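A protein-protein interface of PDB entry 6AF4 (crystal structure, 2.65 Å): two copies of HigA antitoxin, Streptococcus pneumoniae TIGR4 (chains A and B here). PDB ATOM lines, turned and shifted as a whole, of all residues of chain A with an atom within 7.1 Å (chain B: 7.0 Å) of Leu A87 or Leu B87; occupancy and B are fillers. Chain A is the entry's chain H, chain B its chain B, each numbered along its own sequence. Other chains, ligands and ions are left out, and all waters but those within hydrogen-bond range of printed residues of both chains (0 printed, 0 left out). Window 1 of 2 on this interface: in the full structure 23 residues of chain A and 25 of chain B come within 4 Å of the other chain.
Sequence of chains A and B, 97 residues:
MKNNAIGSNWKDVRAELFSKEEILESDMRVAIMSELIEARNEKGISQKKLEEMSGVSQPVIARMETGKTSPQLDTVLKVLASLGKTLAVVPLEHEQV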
ATOM      1  N   LEU A  24       3.362 -28.558  -2.430  1.00  0.00           N
ATOM      2  CA  LEU A  24       3.783 -27.162  -2.472  1.00  0.00           C
ATOM      3  C   LEU A  24       2.573 -26.233  -2.337  1.00  0.00           C
ATOM      4  O   LEU A  24       2.607 -25.262  -1.578  1.00  0.00           O
ATOM      5  CB  LEU A  24       4.544 -26.874  -3.766  1.00  0.00           C
ATOM      6  CG  LEU A  24       5.663 -25.823  -3.764  1.00  0.00           C
ATOM      7  CD1 LEU A  24       6.220 -25.707  -5.169  1.00  0.00           C
ATOM      8  CD2 LEU A  24       5.218 -24.455  -3.240  1.00  0.00           C
ATOM      9  N   MET A  28       1.578 -23.647   0.782  1.00  0.00           N
ATOM     10  CA  MET A  28       1.235 -22.240   0.622  1.00  0.00           C
ATOM     11  C   MET A  28      -0.068 -21.918   1.343  1.00  0.00           C
ATOM     12  O   MET A  28      -0.185 -20.876   1.987  1.00  0.00           O
ATOM     13  CB  MET A  28       1.125 -21.872  -0.860  1.00  0.00           C
ATOM     14  CG  MET A  28       0.754 -20.414  -1.102  1.00  0.00           C
ATOM     15  SD  MET A  28       1.871 -19.261  -0.270  1.00  0.00           S
ATOM     16  CE  MET A  28       3.378 -19.498  -1.208  1.00  0.00           C
ATOM     17  N   ILE A  32      -0.438 -19.299   4.583  1.00  0.00           N
ATOM     18  CA  ILE A  32      -1.399 -18.205   4.619  1.00  0.00           C
ATOM     19  C   ILE A  32      -2.350 -18.354   5.805  1.00  0.00           C
ATOM     20  O   ILE A  32      -2.621 -17.386   6.519  1.00  0.00           O
ATOM     21  CB  ILE A  32      -2.206 -18.138   3.309  1.00  0.00           C
ATOM     22  CG1 ILE A  32      -1.307 -17.678   2.161  1.00  0.00           C
ATOM     23  CG2 ILE A  32      -3.396 -17.210   3.452  1.00  0.00           C
ATOM     24  CD1 ILE A  32      -1.938 -17.843   0.805  1.00  0.00           C
ATOM     25  N   LEU A  73      -3.503 -12.786  -6.515  1.00  0.00           N
ATOM     26  CA  LEU A  73      -2.215 -12.465  -5.994  1.00  0.00           C
ATOM     27  C   LEU A  73      -2.204 -11.131  -5.290  1.00  0.00           C
ATOM     28  O   LEU A  73      -1.453 -10.934  -4.382  1.00  0.00           O
ATOM     29  CB  LEU A  73      -1.223 -12.493  -7.128  1.00  0.00           C
ATOM     30  CG  LEU A  73       0.241 -12.328  -6.815  1.00  0.00           C
ATOM     31  CD1 LEU A  73       0.716 -13.424  -5.887  1.00  0.00           C
ATOM     32  CD2 LEU A  73       0.954 -12.408  -8.144  1.00  0.00           C
ATOM     33  N   VAL A  76      -3.651 -11.282  -1.707  1.00  0.00           N
ATOM     34  CA  VAL A  76      -2.719 -11.982  -0.828  1.00  0.00           C
ATOM     35  C   VAL A  76      -1.596 -11.056  -0.382  1.00  0.00           C
ATOM     36  O   VAL A  76      -1.266 -10.992   0.803  1.00  0.00           O
ATOM     37  CB  VAL A  76      -2.102 -13.224  -1.513  1.00  0.00           C
ATOM     38  CG1 VAL A  76      -1.057 -13.873  -0.613  1.00  0.00           C
ATOM     39  CG2 VAL A  76      -3.180 -14.221  -1.873  1.00  0.00           C
ATOM     40  N   LEU A  77      -1.016 -10.338  -1.340  1.00  0.00           N
ATOM     41  CA  LEU A  77       0.062  -9.395  -1.056  1.00  0.00           C
ATOM     42  C   LEU A  77      -0.403  -8.263  -0.143  1.00  0.00           C
ATOM     43  O   LEU A  77       0.364  -7.779   0.689  1.00  0.00           O
ATOM     44  CB  LEU A  77       0.625  -8.821  -2.359  1.00  0.00           C
ATOM     45  CG  LEU A  77       1.428  -9.778  -3.245  1.00  0.00           C
ATOM     46  CD1 LEU A  77       1.624  -9.191  -4.638  1.00  0.00           C
ATOM     47  CD2 LEU A  77       2.768 -10.105  -2.605  1.00  0.00           C
ATOM     48  N   LEU A  80      -0.970  -9.851   3.471  1.00  0.00           N
ATOM     49  CA  LEU A  80       0.339 -10.155   4.044  1.00  0.00           C
ATOM     50  C   LEU A  80       1.089  -8.892   4.468  1.00  0.00           C
ATOM     51  O   LEU A  80       1.777  -8.884   5.488  1.00  0.00           O
ATOM     52  CB  LEU A  80       1.187 -10.954   3.050  1.00  0.00           C
ATOM     53  CG  LEU A  80       0.797 -12.417   2.824  1.00  0.00           C
ATOM     54  CD1 LEU A  80       1.703 -13.057   1.782  1.00  0.00           C
ATOM     55  CD2 LEU A  80       0.840 -13.199   4.128  1.00  0.00           C
ATOM     56  N   LYS A  85       4.479  -9.415   6.230  1.00  0.00           N
ATOM     57  CA  LYS A  85       5.072 -10.361   5.288  1.00  0.00           C
ATOM     58  C   LYS A  85       4.691 -10.036   3.847  1.00  0.00           C
ATOM     59  O   LYS A  85       3.901  -9.122   3.598  1.00  0.00           O
ATOM     60  CB  LYS A  85       4.646 -11.794   5.620  1.00  0.00           C
ATOM     61  CG  LYS A  85       5.460 -12.459   6.719  1.00  0.00           C
ATOM     62  CD  LYS A  85       4.893 -12.173   8.095  1.00  0.00           C
ATOM     63  CE  LYS A  85       5.647 -12.951   9.160  1.00  0.00           C
ATOM     64  NZ  LYS A  85       4.964 -12.891  10.482  1.00  0.00           N
ATOM     65  N   THR A  86       5.252 -10.798   2.910  1.00  0.00           N
ATOM     66  CA  THR A  86       4.949 -10.664   1.486  1.00  0.00           C
ATOM     67  C   THR A  86       5.584 -11.879   0.783  1.00  0.00           C
ATOM     68  O   THR A  86       6.275 -12.667   1.427  1.00  0.00           O
ATOM     69  CB  THR A  86       5.440  -9.259   0.956  1.00  0.00           C
ATOM     70  OG1 THR A  86       4.382  -8.305   1.125  1.00  0.00           O
ATOM     71  CG2 THR A  86       5.867  -9.239  -0.510  1.00  0.00           C
ATOM     72  N   LEU A  87       5.346 -12.042  -0.516  1.00  0.00           N
ATOM     73  CA  LEU A  87       5.867 -13.168  -1.277  1.00  0.00           C
ATOM     74  C   LEU A  87       7.110 -12.793  -2.075  1.00  0.00           C
ATOM     75  O   LEU A  87       7.250 -11.657  -2.523  1.00  0.00           O
ATOM     76  CB  LEU A  87       4.795 -13.705  -2.222  1.00  0.00           C
ATOM     77  CG  LEU A  87       3.526 -14.233  -1.557  1.00  0.00           C
ATOM     78  CD1 LEU A  87       2.473 -14.555  -2.604  1.00  0.00           C
ATOM     79  CD2 LEU A  87       3.850 -15.460  -0.719  1.00  0.00           C
ATOM     80  N   ALA A  88       8.017 -13.754  -2.228  1.00  0.00           N
ATOM     81  CA  ALA A  88       9.197 -13.578  -3.066  1.00  0.00           C
ATOM     82  C   ALA A  88       9.353 -14.761  -4.012  1.00  0.00           C
ATOM     83  O   ALA A  88       8.909 -15.869  -3.707  1.00  0.00           O
ATOM     84  CB  ALA A  88      10.441 -13.416  -2.209  1.00  0.00           C
ATOM     85  N   VAL A  89       9.977 -14.532  -5.160  1.00  0.00           N
ATOM     86  CA  VAL A  89      10.255 -15.625  -6.082  1.00  0.00           C
ATOM     87  C   VAL A  89      11.576 -16.291  -5.717  1.00  0.00           C
ATOM     88  O   VAL A  89      12.639 -15.673  -5.796  1.00  0.00           O
ATOM     89  CB  VAL A  89      10.312 -15.146  -7.541  1.00  0.00           C
ATOM     90  CG1 VAL A  89      10.766 -16.281  -8.450  1.00  0.00           C
ATOM     91  CG2 VAL A  89       8.959 -14.608  -7.975  1.00  0.00           C
ATOM     92  N   VAL A  90      11.502 -17.559  -5.328  1.00  0.00           N
ATOM     93  CA  VAL A  90      12.674 -18.298  -4.874  1.00  0.00           C
ATOM     94  C   VAL A  90      12.824 -19.598  -5.658  1.00  0.00           C
ATOM     95  O   VAL A  90      11.845 -20.109  -6.203  1.00  0.00           O
ATOM     96  CB  VAL A  90      12.591 -18.615  -3.364  1.00  0.00           C
ATOM     97  CG1 VAL A  90      12.527 -17.332  -2.553  1.00  0.00           C
ATOM     98  CG2 VAL A  90      11.390 -19.501  -3.067  1.00  0.00           C
ATOM     99  N   LEU A  92      13.028 -23.489  -6.581  1.00  0.00           N
ATOM    100  CA  LEU A  92      12.443 -24.731  -6.099  1.00  0.00           C
ATOM    101  C   LEU A  92      13.533 -25.616  -5.495  1.00  0.00           C
ATOM    102  O   LEU A  92      14.685 -25.561  -5.923  1.00  0.00           O
ATOM    103  CB  LEU A  92      11.733 -25.456  -7.244  1.00  0.00           C
ATOM    104  CG  LEU A  92      10.686 -26.499  -6.870  1.00  0.00           C
ATOM    105  CD1 LEU A  92       9.650 -25.868  -5.961  1.00  0.00           C
ATOM    106  CD2 LEU A  92      10.036 -27.062  -8.126  1.00  0.00           C
ATOM    107  N   LEU B  24       5.077  -2.654  -4.627  1.00  0.00           N
ATOM    108  CA  LEU B  24       5.354  -4.020  -4.203  1.00  0.00           C
ATOM    109  C   LEU B  24       4.565  -5.033  -5.033  1.00  0.00           C
ATOM    110  O   LEU B  24       5.115  -6.033  -5.500  1.00  0.00           O
ATOM    111  CB  LEU B  24       5.023  -4.185  -2.719  1.00  0.00           C
ATOM    112  CG  LEU B  24       5.486  -5.461  -2.019  1.00  0.00           C
ATOM    113  CD1 LEU B  24       6.955  -5.361  -1.634  1.00  0.00           C
ATOM    114  CD2 LEU B  24       4.621  -5.728  -0.802  1.00  0.00           C
ATOM    115  N   MET B  28       6.008  -7.814  -8.106  1.00  0.00           N
ATOM    116  CA  MET B  28       5.661  -9.229  -8.037  1.00  0.00           C
ATOM    117  C   MET B  28       5.023  -9.701  -9.338  1.00  0.00           C
ATOM    118  O   MET B  28       5.342 -10.781  -9.836  1.00  0.00           O
ATOM    119  CB  MET B  28       4.725  -9.491  -6.852  1.00  0.00           C
ATOM    120  CG  MET B  28       4.149 -10.903  -6.784  1.00  0.00           C
ATOM    121  SD  MET B  28       5.382 -12.222  -6.840  1.00  0.00           S
ATOM    122  CE  MET B  28       6.494 -11.716  -5.536  1.00  0.00           C
ATOM    123  N   ILE B  32       6.841 -12.472 -12.115  1.00  0.00           N
ATOM    124  CA  ILE B  32       6.179 -13.589 -12.776  1.00  0.00           C
ATOM    125  C   ILE B  32       6.272 -13.446 -14.293  1.00  0.00           C
ATOM    126  O   ILE B  32       6.581 -14.406 -15.000  1.00  0.00           O
ATOM    127  CB  ILE B  32       4.703 -13.694 -12.351  1.00  0.00           C
ATOM    128  CG1 ILE B  32       4.609 -14.139 -10.890  1.00  0.00           C
ATOM    129  CG2 ILE B  32       3.948 -14.665 -13.246  1.00  0.00           C
ATOM    130  CD1 ILE B  32       3.312 -13.748 -10.216  1.00  0.00           C
ATOM    131  N   LEU B  73      -3.480 -17.649  -7.212  1.00  0.00           N
ATOM    132  CA  LEU B  73      -2.254 -18.073  -6.540  1.00  0.00           C
ATOM    133  C   LEU B  73      -1.811 -19.480  -6.926  1.00  0.00           C
ATOM    134  O   LEU B  73      -0.634 -19.705  -7.212  1.00  0.00           O
ATOM    135  CB  LEU B  73      -2.425 -17.989  -5.022  1.00  0.00           C
ATOM    136  CG  LEU B  73      -1.168 -18.251  -4.190  1.00  0.00           C
ATOM    137  CD1 LEU B  73       0.024 -17.484  -4.744  1.00  0.00           C
ATOM    138  CD2 LEU B  73      -1.409 -17.875  -2.740  1.00  0.00           C
ATOM    139  N   VAL B  76      -0.350 -19.558 -10.411  1.00  0.00           N
ATOM    140  CA  VAL B  76       1.010 -19.038 -10.442  1.00  0.00           C
ATOM    141  C   VAL B  76       1.999 -20.091  -9.945  1.00  0.00           C
ATOM    142  O   VAL B  76       3.091 -20.237 -10.494  1.00  0.00           O
ATOM    143  CB  VAL B  76       1.142 -17.757  -9.594  1.00  0.00           C
ATOM    144  CG1 VAL B  76       2.587 -17.305  -9.531  1.00  0.00           C
ATOM    145  CG2 VAL B  76       0.267 -16.654 -10.162  1.00  0.00           C
ATOM    146  N   LEU B  77       1.605 -20.837  -8.917  1.00  0.00           N
ATOM    147  CA  LEU B  77       2.480 -21.847  -8.332  1.00  0.00           C
ATOM    148  C   LEU B  77       2.738 -23.017  -9.282  1.00  0.00           C
ATOM    149  O   LEU B  77       3.841 -23.556  -9.314  1.00  0.00           O
ATOM    150  CB  LEU B  77       1.897 -22.358  -7.015  1.00  0.00           C
ATOM    151  CG  LEU B  77       1.955 -21.357  -5.857  1.00  0.00           C
ATOM    152  CD1 LEU B  77       1.265 -21.921  -4.626  1.00  0.00           C
ATOM    153  CD2 LEU B  77       3.395 -20.967  -5.543  1.00  0.00           C
ATOM    154  N   LEU B  80       5.115 -21.538 -12.136  1.00  0.00           N
ATOM    155  CA  LEU B  80       6.453 -21.292 -11.607  1.00  0.00           C
ATOM    156  C   LEU B  80       7.194 -22.600 -11.326  1.00  0.00           C
ATOM    157  O   LEU B  80       8.393 -22.706 -11.588  1.00  0.00           O
ATOM    158  CB  LEU B  80       6.386 -20.444 -10.334  1.00  0.00           C
ATOM    159  CG  LEU B  80       6.088 -18.947 -10.481  1.00  0.00           C
ATOM    160  CD1 LEU B  80       6.087 -18.268  -9.120  1.00  0.00           C
ATOM    161  CD2 LEU B  80       7.086 -18.274 -11.411  1.00  0.00           C
ATOM    162  N   LYS B  85      10.736 -22.759 -10.152  1.00  0.00           N
ATOM    163  CA  LYS B  85      10.587 -21.652  -9.217  1.00  0.00           C
ATOM    164  C   LYS B  85       9.357 -21.833  -8.338  1.00  0.00           C
ATOM    165  O   LYS B  85       8.499 -22.665  -8.621  1.00  0.00           O
ATOM    166  CB  LYS B  85      10.492 -20.325  -9.974  1.00  0.00           C
ATOM    167  CG  LYS B  85      11.748 -19.940 -10.739  1.00  0.00           C
ATOM    168  CD  LYS B  85      12.807 -19.367  -9.808  1.00  0.00           C
ATOM    169  CE  LYS B  85      14.129 -19.161 -10.533  1.00  0.00           C
ATOM    170  NZ  LYS B  85      13.965 -18.351 -11.772  1.00  0.00           N
ATOM    171  N   THR B  86       9.278 -21.054  -7.267  1.00  0.00           N
ATOM    172  CA  THR B  86       8.069 -21.012  -6.456  1.00  0.00           C
ATOM    173  C   THR B  86       7.988 -19.709  -5.672  1.00  0.00           C
ATOM    174  O   THR B  86       8.835 -18.828  -5.823  1.00  0.00           O
ATOM    175  CB  THR B  86       7.992 -22.199  -5.474  1.00  0.00           C
ATOM    176  OG1 THR B  86       6.702 -22.215  -4.850  1.00  0.00           O
ATOM    177  CG2 THR B  86       9.072 -22.090  -4.404  1.00  0.00           C
ATOM    178  N   LEU B  87       6.958 -19.594  -4.840  1.00  0.00           N
ATOM    179  CA  LEU B  87       6.786 -18.442  -3.967  1.00  0.00           C
ATOM    180  C   LEU B  87       7.011 -18.842  -2.517  1.00  0.00           C
ATOM    181  O   LEU B  87       6.748 -19.978  -2.130  1.00  0.00           O
ATOM    182  CB  LEU B  87       5.389 -17.837  -4.128  1.00  0.00           C
ATOM    183  CG  LEU B  87       4.990 -17.362  -5.525  1.00  0.00           C
ATOM    184  CD1 LEU B  87       3.554 -16.866  -5.526  1.00  0.00           C
ATOM    185  CD2 LEU B  87       5.938 -16.274  -6.017  1.00  0.00           C
ATOM    186  N   ALA B  88       7.498 -17.904  -1.718  1.00  0.00           N
ATOM    187  CA  ALA B  88       7.702 -18.147  -0.300  1.00  0.00           C
ATOM    188  C   ALA B  88       7.259 -16.938   0.508  1.00  0.00           C
ATOM    189  O   ALA B  88       7.434 -15.798   0.074  1.00  0.00           O
ATOM    190  CB  ALA B  88       9.160 -18.465  -0.018  1.00  0.00           C
ATOM    191  N   VAL B  89       6.674 -17.185   1.675  1.00  0.00           N
ATOM    192  CA  VAL B  89       6.381 -16.098   2.593  1.00  0.00           C
ATOM    193  C   VAL B  89       7.704 -15.600   3.174  1.00  0.00           C
ATOM    194  O   VAL B  89       8.562 -16.383   3.586  1.00  0.00           O
ATOM    195  CB  VAL B  89       5.394 -16.524   3.707  1.00  0.00           C
ATOM    196  CG1 VAL B  89       4.108 -17.043   3.088  1.00  0.00           C
ATOM    197  CG2 VAL B  89       6.002 -17.582   4.619  1.00  0.00           C
ATOM    198  N   VAL B  90       7.879 -14.286   3.160  1.00  0.00           N
ATOM    199  CA  VAL B  90       9.144 -13.676   3.538  1.00  0.00           C
ATOM    200  C   VAL B  90       8.841 -12.368   4.270  1.00  0.00           C
ATOM    201  O   VAL B  90       7.836 -11.714   3.979  1.00  0.00           O
ATOM    202  CB  VAL B  90      10.041 -13.446   2.283  1.00  0.00           C
ATOM    203  CG1 VAL B  90       9.471 -12.353   1.394  1.00  0.00           C
ATOM    204  CG2 VAL B  90      11.480 -13.135   2.664  1.00  0.00           C
ATOM    205  N   PRO B  91       9.678 -12.002   5.256  1.00  0.00           N
ATOM    206  CA  PRO B  91       9.459 -10.738   5.972  1.00  0.00           C
ATOM    207  C   PRO B  91       9.458  -9.509   5.062  1.00  0.00           C
ATOM    208  O   PRO B  91       9.997  -9.543   3.956  1.00  0.00           O
ATOM    209  CB  PRO B  91      10.635 -10.687   6.947  1.00  0.00           C
ATOM    210  CG  PRO B  91      10.929 -12.121   7.231  1.00  0.00           C
ATOM    211  CD  PRO B  91      10.660 -12.860   5.947  1.00  0.00           C
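Printed residues of chain B within 4 Å of Leu A87: Met B28, Leu B87 and Ala B88. Of the printed residues of chain B, Val A90 touches Lys B85, Thr B86 and Ala B88. Of the printed residues of chain A, Ile B32 touches Leu A73 (3.4 Å). Printed residues of chain A within 4 Å of Leu B87: Met A28 (3.5 Å), Leu A87 (3.9 Å), Ala A88 (3.3 Å) and Val A89 (3.97 Å). Pro B91 touches none of the printed residues of chain A. The nearest residue of chain B that does not touch Leu A87 is Val B89 (4.1 Å). The nearest printed residue of chain A that does not touch Leu B87 is Val A90 (4.5 Å). The nearest printed residue of chain A that does not touch Ala B88 is Met A28 (4.4 Å).
Met A28 touches Leu B87, and with the chains exchanged Leu A87 touches Met B28. Leu A87 touches Ala B88, and with the chains exchanged Ala A88 touches Leu B87. Ala A88 touches Val B90, and with the chains exchanged Val A90 touches Ala B88. Val A89 touches Lys B85, but with the chains exchanged Lys A85 does not touch Val B89 (5.1 Å). 13 positions are printed for both chains. Of the 26 pairs that touch across the chains among the printed residues, 24 have their exchanged pair printed and touching as well.
Hydrophobic or aromatic side chains of chain B within 4 Å of the printed part of chain A: Leu B24, Met B28, Ile B32, Leu B73, Leu B77, Leu B87, Ala B88 and Val B90. Among the printed residues, no Asp or Glu carboxylate lies within 4 Å of a Lys or Arg side-chain nitrogen of the other chain.
O of Leu B80 is in hydrogen-bond range of N of Lys B85, at 2.7 Å. The backbone NH of Lys A85 is in hydrogen-bond range of the backbone carbonyl oxygen of Leu A80 (2.9 Å).
Among the printed residues, merely in contact across the chains: Leu A24 with Thr B86 (3.1 Å), Met A28 with Leu B73 (3.7 Å), Met A28 with Leu B77 (3.8 Å), Met A28 with Leu B87 (3.5 Å), Ile A32 with Leu B73 (3.6 Å), Leu A73 with Met B28 (3.8 Å), Leu A73 with Ile B32 (3.4 Å), Leu A77 with Met B28 (3.7 Å), Lys A85 with Val B90 (3.3 Å), Thr A86 with Leu B24 (3.2 Å), Thr A86 with Ala B88 (3.6 Å), Thr A86 with Val B89 (3.6 Å), Leu A87 with Met B28 (3.1 Å), Leu A87 with Leu B87 (3.9 Å), Leu A87 with Ala B88 (3.3 Å), Ala A88 with Thr B86 (3.6 Å), Ala A88 with Leu B87 (3.3 Å), Ala A88 with Val B90 (3.9 Å), Val A89 with Lys B85 (3.9 Å), Val A89 with Thr B86 (3.5 Å), Val A89 with Leu B87 (3.97 Å), Val A90 with Lys B85 (3.6 Å) and Val A90 with Ala B88 (3.9 Å).
The backbone NH of Thr B86 sits at hydrogen-bond distance from the backbone carbonyl oxygen of Val A90 (2.9 Å). The backbone NH of Ala A88 lies within hydrogen-bond range of the backbone carbonyl oxygen of Ala B88 (3.1 Å). The backbone NH (N) of Val B90 sits at hydrogen-bond distance from the backbone carbonyl oxygen (O) of Thr A86.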
